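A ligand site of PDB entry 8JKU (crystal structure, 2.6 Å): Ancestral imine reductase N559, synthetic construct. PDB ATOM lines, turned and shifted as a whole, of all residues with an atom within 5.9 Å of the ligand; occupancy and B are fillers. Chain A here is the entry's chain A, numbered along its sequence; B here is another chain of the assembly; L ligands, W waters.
N of Thr 44 lies close to O17 of the ligand (3.0 Å).
O of Thr 77 sits at hydrogen-bond distance from O12 of the ligand.
An oxygen (O12) of the ligand sits at hydrogen-bond distance from the backbone carbonyl oxygen (O) of Val 76 (2.8 Å).
An oxygen (O4) of the ligand lies within hydrogen-bond range of the backbone NH (N) of Thr 77, 3.4 Å away.
The backbone NH of Leu 20 is in hydrogen-bond range of an oxygen (O5) of the ligand.
NZ of Lys 47 is in salt-bridge range of O16 of the ligand.
NH2 of Arg 43 lies within salt-bridge range of O15 of the ligand (3.0 Å).
SG of Cys 75 lies within hydrogen-bond range of O11 of the ligand, at 3.4 Å.
OG1 of Thr 44 is in hydrogen-bond range of O17 of the ligand, at 2.9 Å.
N of Met 23 lies within hydrogen-bond range of O9 of the ligand, at 3.3 Å.
The backbone NH of Ser 103 lies within hydrogen-bond range of an oxygen (O12) of the ligand.
The side-chain amide oxygen (OD1) of Asn 42 lies within hydrogen-bond range of an oxygen (O5) of the ligand (2.9 Å).
O3 of the ligand sits at hydrogen-bond distance from OG1 of Thr 77, 3.1 Å away.
The backbone NH (N) of Gly 21 is in hydrogen-bond range of an oxygen (O5) of the ligand (3.2 Å).
The side-chain amide oxygen (OD1) of Asn 42 lies within hydrogen-bond range of the backbone NH (N) of Leu 20, 2.9 Å away.
The backbone carbonyl oxygen (O) of Thr 44 sits at hydrogen-bond distance from the side-chain amide nitrogen (ND2) of Asn 42 (3.0 Å).
The side-chain hydroxyl (OG1) of Thr 102 sits at hydrogen-bond distance from the backbone NH (N) of Val 76.
N of Ala 81 is in hydrogen-bond range of OD1 of Asp 78 (3.1 Å).
The backbone carbonyl oxygen (O) of Trp 41 lies within hydrogen-bond range of the backbone NH (N) of Gly 19, at 2.8 Å.
The backbone nitrogen (N) of Pro 22 lies close to an oxygen (O9) of the ligand.
C of Gly 19 touches O5 of the ligand, at 3.6 Å.
CB of Ala 81 touches C7 of the ligand (3.6 Å).
Ile 85 touches the ligand.
Thr 102 touches the ligand.
Ile 128 touches the ligand (O to C20, 3.1 Å).
Val 130 touches the ligand (O to C19, 3.1 Å).
Pro 131 touches the ligand.
Pro 132 touches the ligand.
Of the 29 residues printed, 20 come within 4 Å of the ligand.
Water W1 lies within hydrogen-bond range of O of Cys 75 (2.7 Å), O9 of the ligand (2.7 Å), N of Gly 24 (2.8 Å) and N of Gly 21 (3.2 Å).
Water W2 lies within hydrogen-bond range of OD1 of Asn 42, N5 of the ligand and N of Arg 43.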
ATOM      1  N   GLY A  19       0.917   8.892  -8.860  1.00  0.00           N
ATOM      2  CA  GLY A  19       1.619   9.091 -10.119  1.00  0.00           C
ATOM      3  C   GLY A  19       0.703   9.585 -11.207  1.00  0.00           C
ATOM      4  O   GLY A  19      -0.214   8.872 -11.621  1.00  0.00           O
ATOM      5  N   LEU A  20       0.939  10.810 -11.680  1.00  0.00           N
ATOM      6  CA  LEU A  20       0.052  11.423 -12.666  1.00  0.00           C
ATOM      7  C   LEU A  20       0.779  11.680 -13.984  1.00  0.00           C
ATOM      8  O   LEU A  20       0.752  12.803 -14.511  1.00  0.00           O
ATOM      9  CB  LEU A  20      -0.537  12.723 -12.118  1.00  0.00           C
ATOM     10  CG  LEU A  20      -1.558  12.569 -10.993  1.00  0.00           C
ATOM     11  CD1 LEU A  20      -2.149  13.932 -10.621  1.00  0.00           C
ATOM     12  CD2 LEU A  20      -2.664  11.599 -11.384  1.00  0.00           C
ATOM     13  N   GLY A  21       1.439  10.662 -14.514  1.00  0.00           N
ATOM     14  CA  GLY A  21       1.976  10.725 -15.843  1.00  0.00           C
ATOM     15  C   GLY A  21       0.906  10.428 -16.860  1.00  0.00           C
ATOM     16  O   GLY A  21      -0.276  10.304 -16.525  1.00  0.00           O
ATOM     17  N   PRO A  22       1.284  10.303 -18.134  1.00  0.00           N
ATOM     18  CA  PRO A  22       0.282   9.979 -19.167  1.00  0.00           C
ATOM     19  C   PRO A  22      -0.643   8.834 -18.783  1.00  0.00           C
ATOM     20  O   PRO A  22      -1.865   8.950 -18.918  1.00  0.00           O
ATOM     21  CB  PRO A  22       1.151   9.637 -20.394  1.00  0.00           C
ATOM     22  CG  PRO A  22       2.407  10.452 -20.205  1.00  0.00           C
ATOM     23  CD  PRO A  22       2.633  10.543 -18.699  1.00  0.00           C
ATOM     24  N   MET A  23      -0.083   7.723 -18.298  1.00  0.00           N
ATOM     25  CA  MET A  23      -0.918   6.579 -17.931  1.00  0.00           C
ATOM     26  C   MET A  23      -1.631   6.816 -16.609  1.00  0.00           C
ATOM     27  O   MET A  23      -2.833   6.559 -16.492  1.00  0.00           O
ATOM     28  CB  MET A  23      -0.057   5.314 -17.859  1.00  0.00           C
ATOM     29  CG  MET A  23      -0.863   4.030 -17.741  1.00  0.00           C
ATOM     30  SD  MET A  23      -2.024   3.776 -19.099  1.00  0.00           S
ATOM     31  CE  MET A  23      -0.924   3.202 -20.383  1.00  0.00           C
ATOM     32  N   GLY A  24      -0.900   7.292 -15.604  1.00  0.00           N
ATOM     33  CA  GLY A  24      -1.527   7.567 -14.318  1.00  0.00           C
ATOM     34  C   GLY A  24      -2.706   8.509 -14.440  1.00  0.00           C
ATOM     35  O   GLY A  24      -3.729   8.323 -13.774  1.00  0.00           O
ATOM     36  N   TRP A  41      -2.259  11.968  -6.625  1.00  0.00           N
ATOM     37  CA  TRP A  41      -1.059  12.602  -6.107  1.00  0.00           C
ATOM     38  C   TRP A  41       0.062  12.422  -7.124  1.00  0.00           C
ATOM     39  O   TRP A  41       0.127  11.393  -7.818  1.00  0.00           O
ATOM     40  CB  TRP A  41      -0.635  12.028  -4.753  1.00  0.00           C
ATOM     41  CG  TRP A  41       0.629  12.668  -4.229  1.00  0.00           C
ATOM     42  CD1 TRP A  41       0.719  13.760  -3.414  1.00  0.00           C
ATOM     43  CD2 TRP A  41       1.972  12.251  -4.498  1.00  0.00           C
ATOM     44  NE1 TRP A  41       2.035  14.056  -3.161  1.00  0.00           N
ATOM     45  CE2 TRP A  41       2.825  13.144  -3.811  1.00  0.00           C
ATOM     46  CE3 TRP A  41       2.541  11.222  -5.258  1.00  0.00           C
ATOM     47  CZ2 TRP A  41       4.214  13.024  -3.860  1.00  0.00           C
ATOM     48  CZ3 TRP A  41       3.915  11.110  -5.304  1.00  0.00           C
ATOM     49  CH2 TRP A  41       4.737  12.002  -4.606  1.00  0.00           C
ATOM     50  N   ASN A  42       0.948  13.413  -7.194  1.00  0.00           N
ATOM     51  CA  ASN A  42       2.088  13.378  -8.098  1.00  0.00           C
ATOM     52  C   ASN A  42       3.236  14.150  -7.472  1.00  0.00           C
ATOM     53  O   ASN A  42       3.026  15.049  -6.660  1.00  0.00           O
ATOM     54  CB  ASN A  42       1.738  13.962  -9.467  1.00  0.00           C
ATOM     55  CG  ASN A  42       2.710  13.523 -10.551  1.00  0.00           C
ATOM     56  OD1 ASN A  42       3.130  12.366 -10.589  1.00  0.00           O
ATOM     57  ND2 ASN A  42       3.075  14.443 -11.438  1.00  0.00           N
ATOM     58  N   ARG A  43       4.459  13.781  -7.870  1.00  0.00           N
ATOM     59  CA  ARG A  43       5.632  14.510  -7.404  1.00  0.00           C
ATOM     60  C   ARG A  43       5.683  15.901  -8.011  1.00  0.00           C
ATOM     61  O   ARG A  43       5.993  16.879  -7.319  1.00  0.00           O
ATOM     62  CB  ARG A  43       6.898  13.713  -7.728  1.00  0.00           C
ATOM     63  CG  ARG A  43       8.133  14.556  -8.019  1.00  0.00           C
ATOM     64  CD  ARG A  43       9.312  13.681  -8.444  1.00  0.00           C
ATOM     65  NE  ARG A  43       9.206  13.301  -9.847  1.00  0.00           N
ATOM     66  CZ  ARG A  43      10.236  12.994 -10.618  1.00  0.00           C
ATOM     67  NH1 ARG A  43      11.471  12.993 -10.155  1.00  0.00           N
ATOM     68  NH2 ARG A  43      10.020  12.684 -11.902  1.00  0.00           N
ATOM     69  N   THR A  44       5.397  16.019  -9.303  1.00  0.00           N
ATOM     70  CA  THR A  44       5.406  17.304  -9.979  1.00  0.00           C
ATOM     71  C   THR A  44       4.006  17.890  -9.979  1.00  0.00           C
ATOM     72  O   THR A  44       3.082  17.260 -10.511  1.00  0.00           O
ATOM     73  CB  THR A  44       5.909  17.163 -11.412  1.00  0.00           C
ATOM     74  OG1 THR A  44       7.310  16.867 -11.402  1.00  0.00           O
ATOM     75  CG2 THR A  44       5.652  18.428 -12.205  1.00  0.00           C
ATOM     76  N   LYS A  47      -0.597  18.813 -12.893  1.00  0.00           N
ATOM     77  CA  LYS A  47      -1.021  17.844 -13.885  1.00  0.00           C
ATOM     78  C   LYS A  47      -2.412  17.277 -13.633  1.00  0.00           C
ATOM     79  O   LYS A  47      -2.849  16.407 -14.384  1.00  0.00           O
ATOM     80  CB  LYS A  47      -0.025  16.677 -13.955  1.00  0.00           C
ATOM     81  CG  LYS A  47       1.431  17.097 -14.091  1.00  0.00           C
ATOM     82  CD  LYS A  47       2.271  15.940 -14.610  1.00  0.00           C
ATOM     83  CE  LYS A  47       3.756  16.270 -14.594  1.00  0.00           C
ATOM     84  NZ  LYS A  47       4.524  15.397 -15.530  1.00  0.00           N
ATOM     85  N   CYS A  75       1.355   4.072 -10.507  1.00  0.00           N
ATOM     86  CA  CYS A  75       1.765   3.970 -11.910  1.00  0.00           C
ATOM     87  C   CYS A  75       2.889   4.975 -12.157  1.00  0.00           C
ATOM     88  O   CYS A  75       2.635   6.098 -12.593  1.00  0.00           O
ATOM     89  CB  CYS A  75       0.577   4.214 -12.843  1.00  0.00           C
ATOM     90  SG  CYS A  75       0.910   3.778 -14.561  1.00  0.00           S
ATOM     91  N   VAL A  76       4.118   4.555 -11.889  1.00  0.00           N
ATOM     92  CA  VAL A  76       5.287   5.392 -12.099  1.00  0.00           C
ATOM     93  C   VAL A  76       6.214   4.706 -13.090  1.00  0.00           C
ATOM     94  O   VAL A  76       5.872   3.657 -13.654  1.00  0.00           O
ATOM     95  CB  VAL A  76       6.013   5.684 -10.768  1.00  0.00           C
ATOM     96  CG1 VAL A  76       5.157   6.589  -9.896  1.00  0.00           C
ATOM     97  CG2 VAL A  76       6.348   4.392 -10.041  1.00  0.00           C
ATOM     98  N   THR A  77       7.396   5.278 -13.307  1.00  0.00           N
ATOM     99  CA  THR A  77       8.277   4.796 -14.369  1.00  0.00           C
ATOM    100  C   THR A  77       8.775   3.380 -14.094  1.00  0.00           C
ATOM    101  O   THR A  77       8.573   2.462 -14.899  1.00  0.00           O
ATOM    102  CB  THR A  77       9.460   5.752 -14.551  1.00  0.00           C
ATOM    103  OG1 THR A  77       9.010   6.983 -15.131  1.00  0.00           O
ATOM    104  CG2 THR A  77      10.532   5.136 -15.435  1.00  0.00           C
ATOM    105  N   ASP A  78       9.448   3.192 -12.968  1.00  0.00           N
ATOM    106  CA  ASP A  78       9.986   1.894 -12.572  1.00  0.00           C
ATOM    107  C   ASP A  78       9.627   1.654 -11.110  1.00  0.00           C
ATOM    108  O   ASP A  78       9.001   2.483 -10.446  1.00  0.00           O
ATOM    109  CB  ASP A  78      11.500   1.823 -12.784  1.00  0.00           C
ATOM    110  CG  ASP A  78      12.191   3.141 -12.471  1.00  0.00           C
ATOM    111  OD1 ASP A  78      11.645   3.917 -11.663  1.00  0.00           O
ATOM    112  OD2 ASP A  78      13.273   3.389 -13.036  1.00  0.00           O
ATOM    113  N   ASP A  80      11.925   1.312  -8.751  1.00  0.00           N
ATOM    114  CA  ASP A  80      12.799   2.193  -7.989  1.00  0.00           C
ATOM    115  C   ASP A  80      12.089   3.492  -7.625  1.00  0.00           C
ATOM    116  O   ASP A  80      12.250   4.015  -6.514  1.00  0.00           O
ATOM    117  CB  ASP A  80      14.078   2.498  -8.785  1.00  0.00           C
ATOM    118  CG  ASP A  80      14.978   1.293  -8.910  1.00  0.00           C
ATOM    119  OD1 ASP A  80      15.046   0.485  -7.965  1.00  0.00           O
ATOM    120  OD2 ASP A  80      15.624   1.150  -9.979  1.00  0.00           O
ATOM    121  N   ALA A  81      11.284   4.011  -8.549  1.00  0.00           N
ATOM    122  CA  ALA A  81      10.490   5.204  -8.261  1.00  0.00           C
ATOM    123  C   ALA A  81       9.319   4.858  -7.350  1.00  0.00           C
ATOM    124  O   ALA A  81       9.013   5.600  -6.407  1.00  0.00           O
ATOM    125  CB  ALA A  81       9.996   5.826  -9.558  1.00  0.00           C
ATOM    126  N   ALA A  84      10.563   4.624  -3.945  1.00  0.00           N
ATOM    127  CA  ALA A  84      10.990   5.916  -3.426  1.00  0.00           C
ATOM    128  C   ALA A  84       9.804   6.776  -3.032  1.00  0.00           C
ATOM    129  O   ALA A  84       9.883   7.539  -2.070  1.00  0.00           O
ATOM    130  CB  ALA A  84      11.856   6.639  -4.463  1.00  0.00           C
ATOM    131  N   ILE A  85       8.696   6.667  -3.765  1.00  0.00           N
ATOM    132  CA  ILE A  85       7.522   7.483  -3.464  1.00  0.00           C
ATOM    133  C   ILE A  85       6.778   6.932  -2.259  1.00  0.00           C
ATOM    134  O   ILE A  85       6.247   7.700  -1.454  1.00  0.00           O
ATOM    135  CB  ILE A  85       6.606   7.550  -4.699  1.00  0.00           C
ATOM    136  CG1 ILE A  85       7.310   8.238  -5.863  1.00  0.00           C
ATOM    137  CG2 ILE A  85       5.304   8.277  -4.371  1.00  0.00           C
ATOM    138  CD1 ILE A  85       6.529   8.205  -7.154  1.00  0.00           C
ATOM    139  N   LEU A 101       0.766  -1.023 -11.066  1.00  0.00           N
ATOM    140  CA  LEU A 101       0.673  -1.006 -12.521  1.00  0.00           C
ATOM    141  C   LEU A 101       1.918  -0.417 -13.167  1.00  0.00           C
ATOM    142  O   LEU A 101       1.884  -0.014 -14.334  1.00  0.00           O
ATOM    143  CB  LEU A 101      -0.579  -0.238 -12.954  1.00  0.00           C
ATOM    144  CG  LEU A 101      -1.902  -0.759 -12.387  1.00  0.00           C
ATOM    145  CD1 LEU A 101      -3.078  -0.214 -13.185  1.00  0.00           C
ATOM    146  CD2 LEU A 101      -1.940  -2.278 -12.379  1.00  0.00           C
ATOM    147  N   THR A 102       3.015  -0.345 -12.418  1.00  0.00           N
ATOM    148  CA  THR A 102       4.304   0.032 -12.982  1.00  0.00           C
ATOM    149  C   THR A 102       4.933  -1.176 -13.667  1.00  0.00           C
ATOM    150  O   THR A 102       4.835  -2.302 -13.166  1.00  0.00           O
ATOM    151  CB  THR A 102       5.227   0.563 -11.891  1.00  0.00           C
ATOM    152  OG1 THR A 102       4.615   1.694 -11.250  1.00  0.00           O
ATOM    153  CG2 THR A 102       6.569   0.986 -12.473  1.00  0.00           C
ATOM    154  N   SER A 103       5.562  -0.943 -14.817  1.00  0.00           N
ATOM    155  CA  SER A 103       6.137  -2.012 -15.605  1.00  0.00           C
ATOM    156  C   SER A 103       7.587  -2.230 -15.191  1.00  0.00           C
ATOM    157  O   SER A 103       8.393  -1.298 -15.213  1.00  0.00           O
ATOM    158  CB  SER A 103       6.055  -1.680 -17.101  1.00  0.00           C
ATOM    159  OG  SER A 103       4.841  -2.155 -17.672  1.00  0.00           O
ATOM    160  N   ILE A 128       0.009  -2.970 -17.788  1.00  0.00           N
ATOM    161  CA  ILE A 128      -0.842  -2.366 -18.808  1.00  0.00           C
ATOM    162  C   ILE A 128      -0.208  -2.612 -20.169  1.00  0.00           C
ATOM    163  O   ILE A 128       0.924  -2.211 -20.416  1.00  0.00           O
ATOM    164  CB  ILE A 128      -1.038  -0.865 -18.545  1.00  0.00           C
ATOM    165  CG1 ILE A 128      -1.864  -0.649 -17.270  1.00  0.00           C
ATOM    166  CG2 ILE A 128      -1.719  -0.210 -19.737  1.00  0.00           C
ATOM    167  CD1 ILE A 128      -1.454   0.570 -16.478  1.00  0.00           C
ATOM    168  N   MET A 129      -0.959  -3.268 -21.062  1.00  0.00           N
ATOM    169  CA  MET A 129      -0.460  -3.623 -22.387  1.00  0.00           C
ATOM    170  C   MET A 129      -1.048  -2.740 -23.481  1.00  0.00           C
ATOM    171  O   MET A 129      -1.019  -3.116 -24.652  1.00  0.00           O
ATOM    172  CB  MET A 129      -0.754  -5.086 -22.688  1.00  0.00           C
ATOM    173  CG  MET A 129      -0.175  -6.091 -21.685  1.00  0.00           C
ATOM    174  SD  MET A 129       1.528  -5.783 -21.208  1.00  0.00           S
ATOM    175  CE  MET A 129       2.370  -5.995 -22.780  1.00  0.00           C
ATOM    176  N   VAL A 130      -1.581  -1.576 -23.130  1.00  0.00           N
ATOM    177  CA  VAL A 130      -2.182  -0.653 -24.091  1.00  0.00           C
ATOM    178  C   VAL A 130      -1.735   0.760 -23.790  1.00  0.00           C
ATOM    179  O   VAL A 130      -1.252   1.051 -22.684  1.00  0.00           O
ATOM    180  CB  VAL A 130      -3.725  -0.727 -24.081  1.00  0.00           C
ATOM    181  CG1 VAL A 130      -4.194  -2.131 -24.415  1.00  0.00           C
ATOM    182  CG2 VAL A 130      -4.254  -0.279 -22.720  1.00  0.00           C
ATOM    183  N   PRO A 131      -1.882   1.678 -24.749  1.00  0.00           N
ATOM    184  CA  PRO A 131      -1.549   3.077 -24.488  1.00  0.00           C
ATOM    185  C   PRO A 131      -2.646   3.766 -23.696  1.00  0.00           C
ATOM    186  O   PRO A 131      -3.775   3.253 -23.603  1.00  0.00           O
ATOM    187  CB  PRO A 131      -1.415   3.677 -25.896  1.00  0.00           C
ATOM    188  CG  PRO A 131      -2.308   2.834 -26.749  1.00  0.00           C
ATOM    189  CD  PRO A 131      -2.285   1.436 -26.151  1.00  0.00           C
ATOM    190  N   PRO A 132      -2.355   4.920 -23.100  1.00  0.00           N
ATOM    191  CA  PRO A 132      -3.330   5.562 -22.196  1.00  0.00           C
ATOM    192  C   PRO A 132      -4.674   5.792 -22.848  1.00  0.00           C
ATOM    193  O   PRO A 132      -5.717   5.524 -22.229  1.00  0.00           O
ATOM    194  CB  PRO A 132      -2.642   6.892 -21.830  1.00  0.00           C
ATOM    195  CG  PRO A 132      -1.177   6.610 -21.967  1.00  0.00           C
ATOM    196  CD  PRO A 132      -1.045   5.607 -23.102  1.00  0.00           C
ATOM    197  N   SER B 240       6.206   7.515 -26.853  1.00  0.00           N
ATOM    198  CA  SER B 240       7.215   6.469 -26.778  1.00  0.00           C
ATOM    199  C   SER B 240       8.502   6.896 -27.483  1.00  0.00           C
ATOM    200  O   SER B 240       8.498   7.189 -28.681  1.00  0.00           O
ATOM    201  CB  SER B 240       6.694   5.176 -27.405  1.00  0.00           C
ATOM    202  OG  SER B 240       6.900   4.069 -26.548  1.00  0.00           O
ATOM    203  N   MET B 244      13.204   5.328 -23.567  1.00  0.00           N
ATOM    204  CA  MET B 244      12.330   4.506 -22.739  1.00  0.00           C
ATOM    205  C   MET B 244      12.298   3.060 -23.235  1.00  0.00           C
ATOM    206  O   MET B 244      12.541   2.122 -22.469  1.00  0.00           O
ATOM    207  CB  MET B 244      10.912   5.099 -22.719  1.00  0.00           C
ATOM    208  CG  MET B 244      10.875   6.616 -22.565  1.00  0.00           C
ATOM    209  SD  MET B 244       9.294   7.231 -21.982  1.00  0.00           S
ATOM    210  CE  MET B 244       8.396   7.350 -23.530  1.00  0.00           C
HETATM  211  P1  LIG L   1       6.589   7.292 -17.261  1.00  0.00           P
HETATM  212  O1  LIG L   1       7.554   8.377 -17.586  1.00  0.00           O
HETATM  213  O2  LIG L   1       7.045   5.884 -17.389  1.00  0.00           O
HETATM  214  O3  LIG L   1       5.999   7.534 -15.798  1.00  0.00           O
HETATM  215  C1  LIG L   1       5.592   8.876 -15.479  1.00  0.00           C
HETATM  216  C2  LIG L   1       5.244   8.987 -14.022  1.00  0.00           C
HETATM  217  O4  LIG L   1       6.338   8.462 -13.217  1.00  0.00           O
HETATM  218  C3  LIG L   1       5.016  10.412 -13.519  1.00  0.00           C
HETATM  219  O5  LIG L   1       3.962  10.467 -12.573  1.00  0.00           O
HETATM  220  C4  LIG L   1       6.376  10.738 -12.915  1.00  0.00           C
HETATM  221  O6  LIG L   1       6.374  11.790 -11.960  1.00  0.00           O
HETATM  222  C5  LIG L   1       6.618   9.420 -12.224  1.00  0.00           C
HETATM  223  N1  LIG L   1       7.979   9.257 -11.733  1.00  0.00           N
HETATM  224  C6  LIG L   1       9.064   8.738 -12.401  1.00  0.00           C
HETATM  225  N2  LIG L   1      10.154   8.720 -11.685  1.00  0.00           N
HETATM  226  C7  LIG L   1       9.776   9.257 -10.470  1.00  0.00           C
HETATM  227  C8  LIG L   1      10.487   9.510  -9.277  1.00  0.00           C
HETATM  228  N3  LIG L   1      11.780   9.231  -9.124  1.00  0.00           N
HETATM  229  N4  LIG L   1       9.807  10.048  -8.252  1.00  0.00           N
HETATM  230  C9  LIG L   1       8.510  10.323  -8.417  1.00  0.00           C
HETATM  231  N5  LIG L   1       7.736  10.130  -9.480  1.00  0.00           N
HETATM  232  C10 LIG L   1       8.440   9.591 -10.483  1.00  0.00           C
HETATM  233  O7  LIG L   1       5.287   7.497 -18.165  1.00  0.00           O
HETATM  234  P2  LIG L   1       3.794   6.901 -18.157  1.00  0.00           P
HETATM  235  O8  LIG L   1       3.271   6.894 -19.550  1.00  0.00           O
HETATM  236  O9  LIG L   1       3.015   7.597 -17.113  1.00  0.00           O
HETATM  237  O10 LIG L   1       4.085   5.399 -17.700  1.00  0.00           O
HETATM  238  C11 LIG L   1       3.651   4.983 -16.391  1.00  0.00           C
HETATM  239  C12 LIG L   1       3.887   3.495 -16.281  1.00  0.00           C
HETATM  240  O11 LIG L   1       2.938   2.803 -17.114  1.00  0.00           O
HETATM  241  C13 LIG L   1       5.284   3.028 -16.710  1.00  0.00           C
HETATM  242  O12 LIG L   1       5.775   1.995 -15.879  1.00  0.00           O
HETATM  243  C14 LIG L   1       5.049   2.511 -18.141  1.00  0.00           C
HETATM  244  O13 LIG L   1       5.926   1.459 -18.487  1.00  0.00           O
HETATM  245  C15 LIG L   1       3.635   1.949 -18.023  1.00  0.00           C
HETATM  246  N6  LIG L   1       2.902   1.929 -19.305  1.00  0.00           N
HETATM  247  C16 LIG L   1       2.837   3.071 -20.074  1.00  0.00           C
HETATM  248  C17 LIG L   1       2.164   3.052 -21.291  1.00  0.00           C
HETATM  249  C18 LIG L   1       2.076   4.279 -22.134  1.00  0.00           C
HETATM  250  O14 LIG L   1       2.119   5.398 -21.593  1.00  0.00           O
HETATM  251  N7  LIG L   1       1.949   4.127 -23.445  1.00  0.00           N
HETATM  252  C19 LIG L   1       1.553   1.882 -21.728  1.00  0.00           C
HETATM  253  C20 LIG L   1       1.621   0.753 -20.940  1.00  0.00           C
HETATM  254  C21 LIG L   1       2.305   0.785 -19.738  1.00  0.00           C
HETATM  255  P3  LIG L   1       6.363  13.226 -12.661  1.00  0.00           P
HETATM  256  O15 LIG L   1       7.560  13.409 -13.546  1.00  0.00           O
HETATM  257  O16 LIG L   1       5.090  13.287 -13.443  1.00  0.00           O
HETATM  258  O17 LIG L   1       6.373  14.174 -11.505  1.00  0.00           O
HETATM  259  O   HOH W   1       1.715   7.512 -14.700  1.00  0.00           O
HETATM  260  O   HOH W   2       5.161  11.079  -9.255  1.00  0.00           O
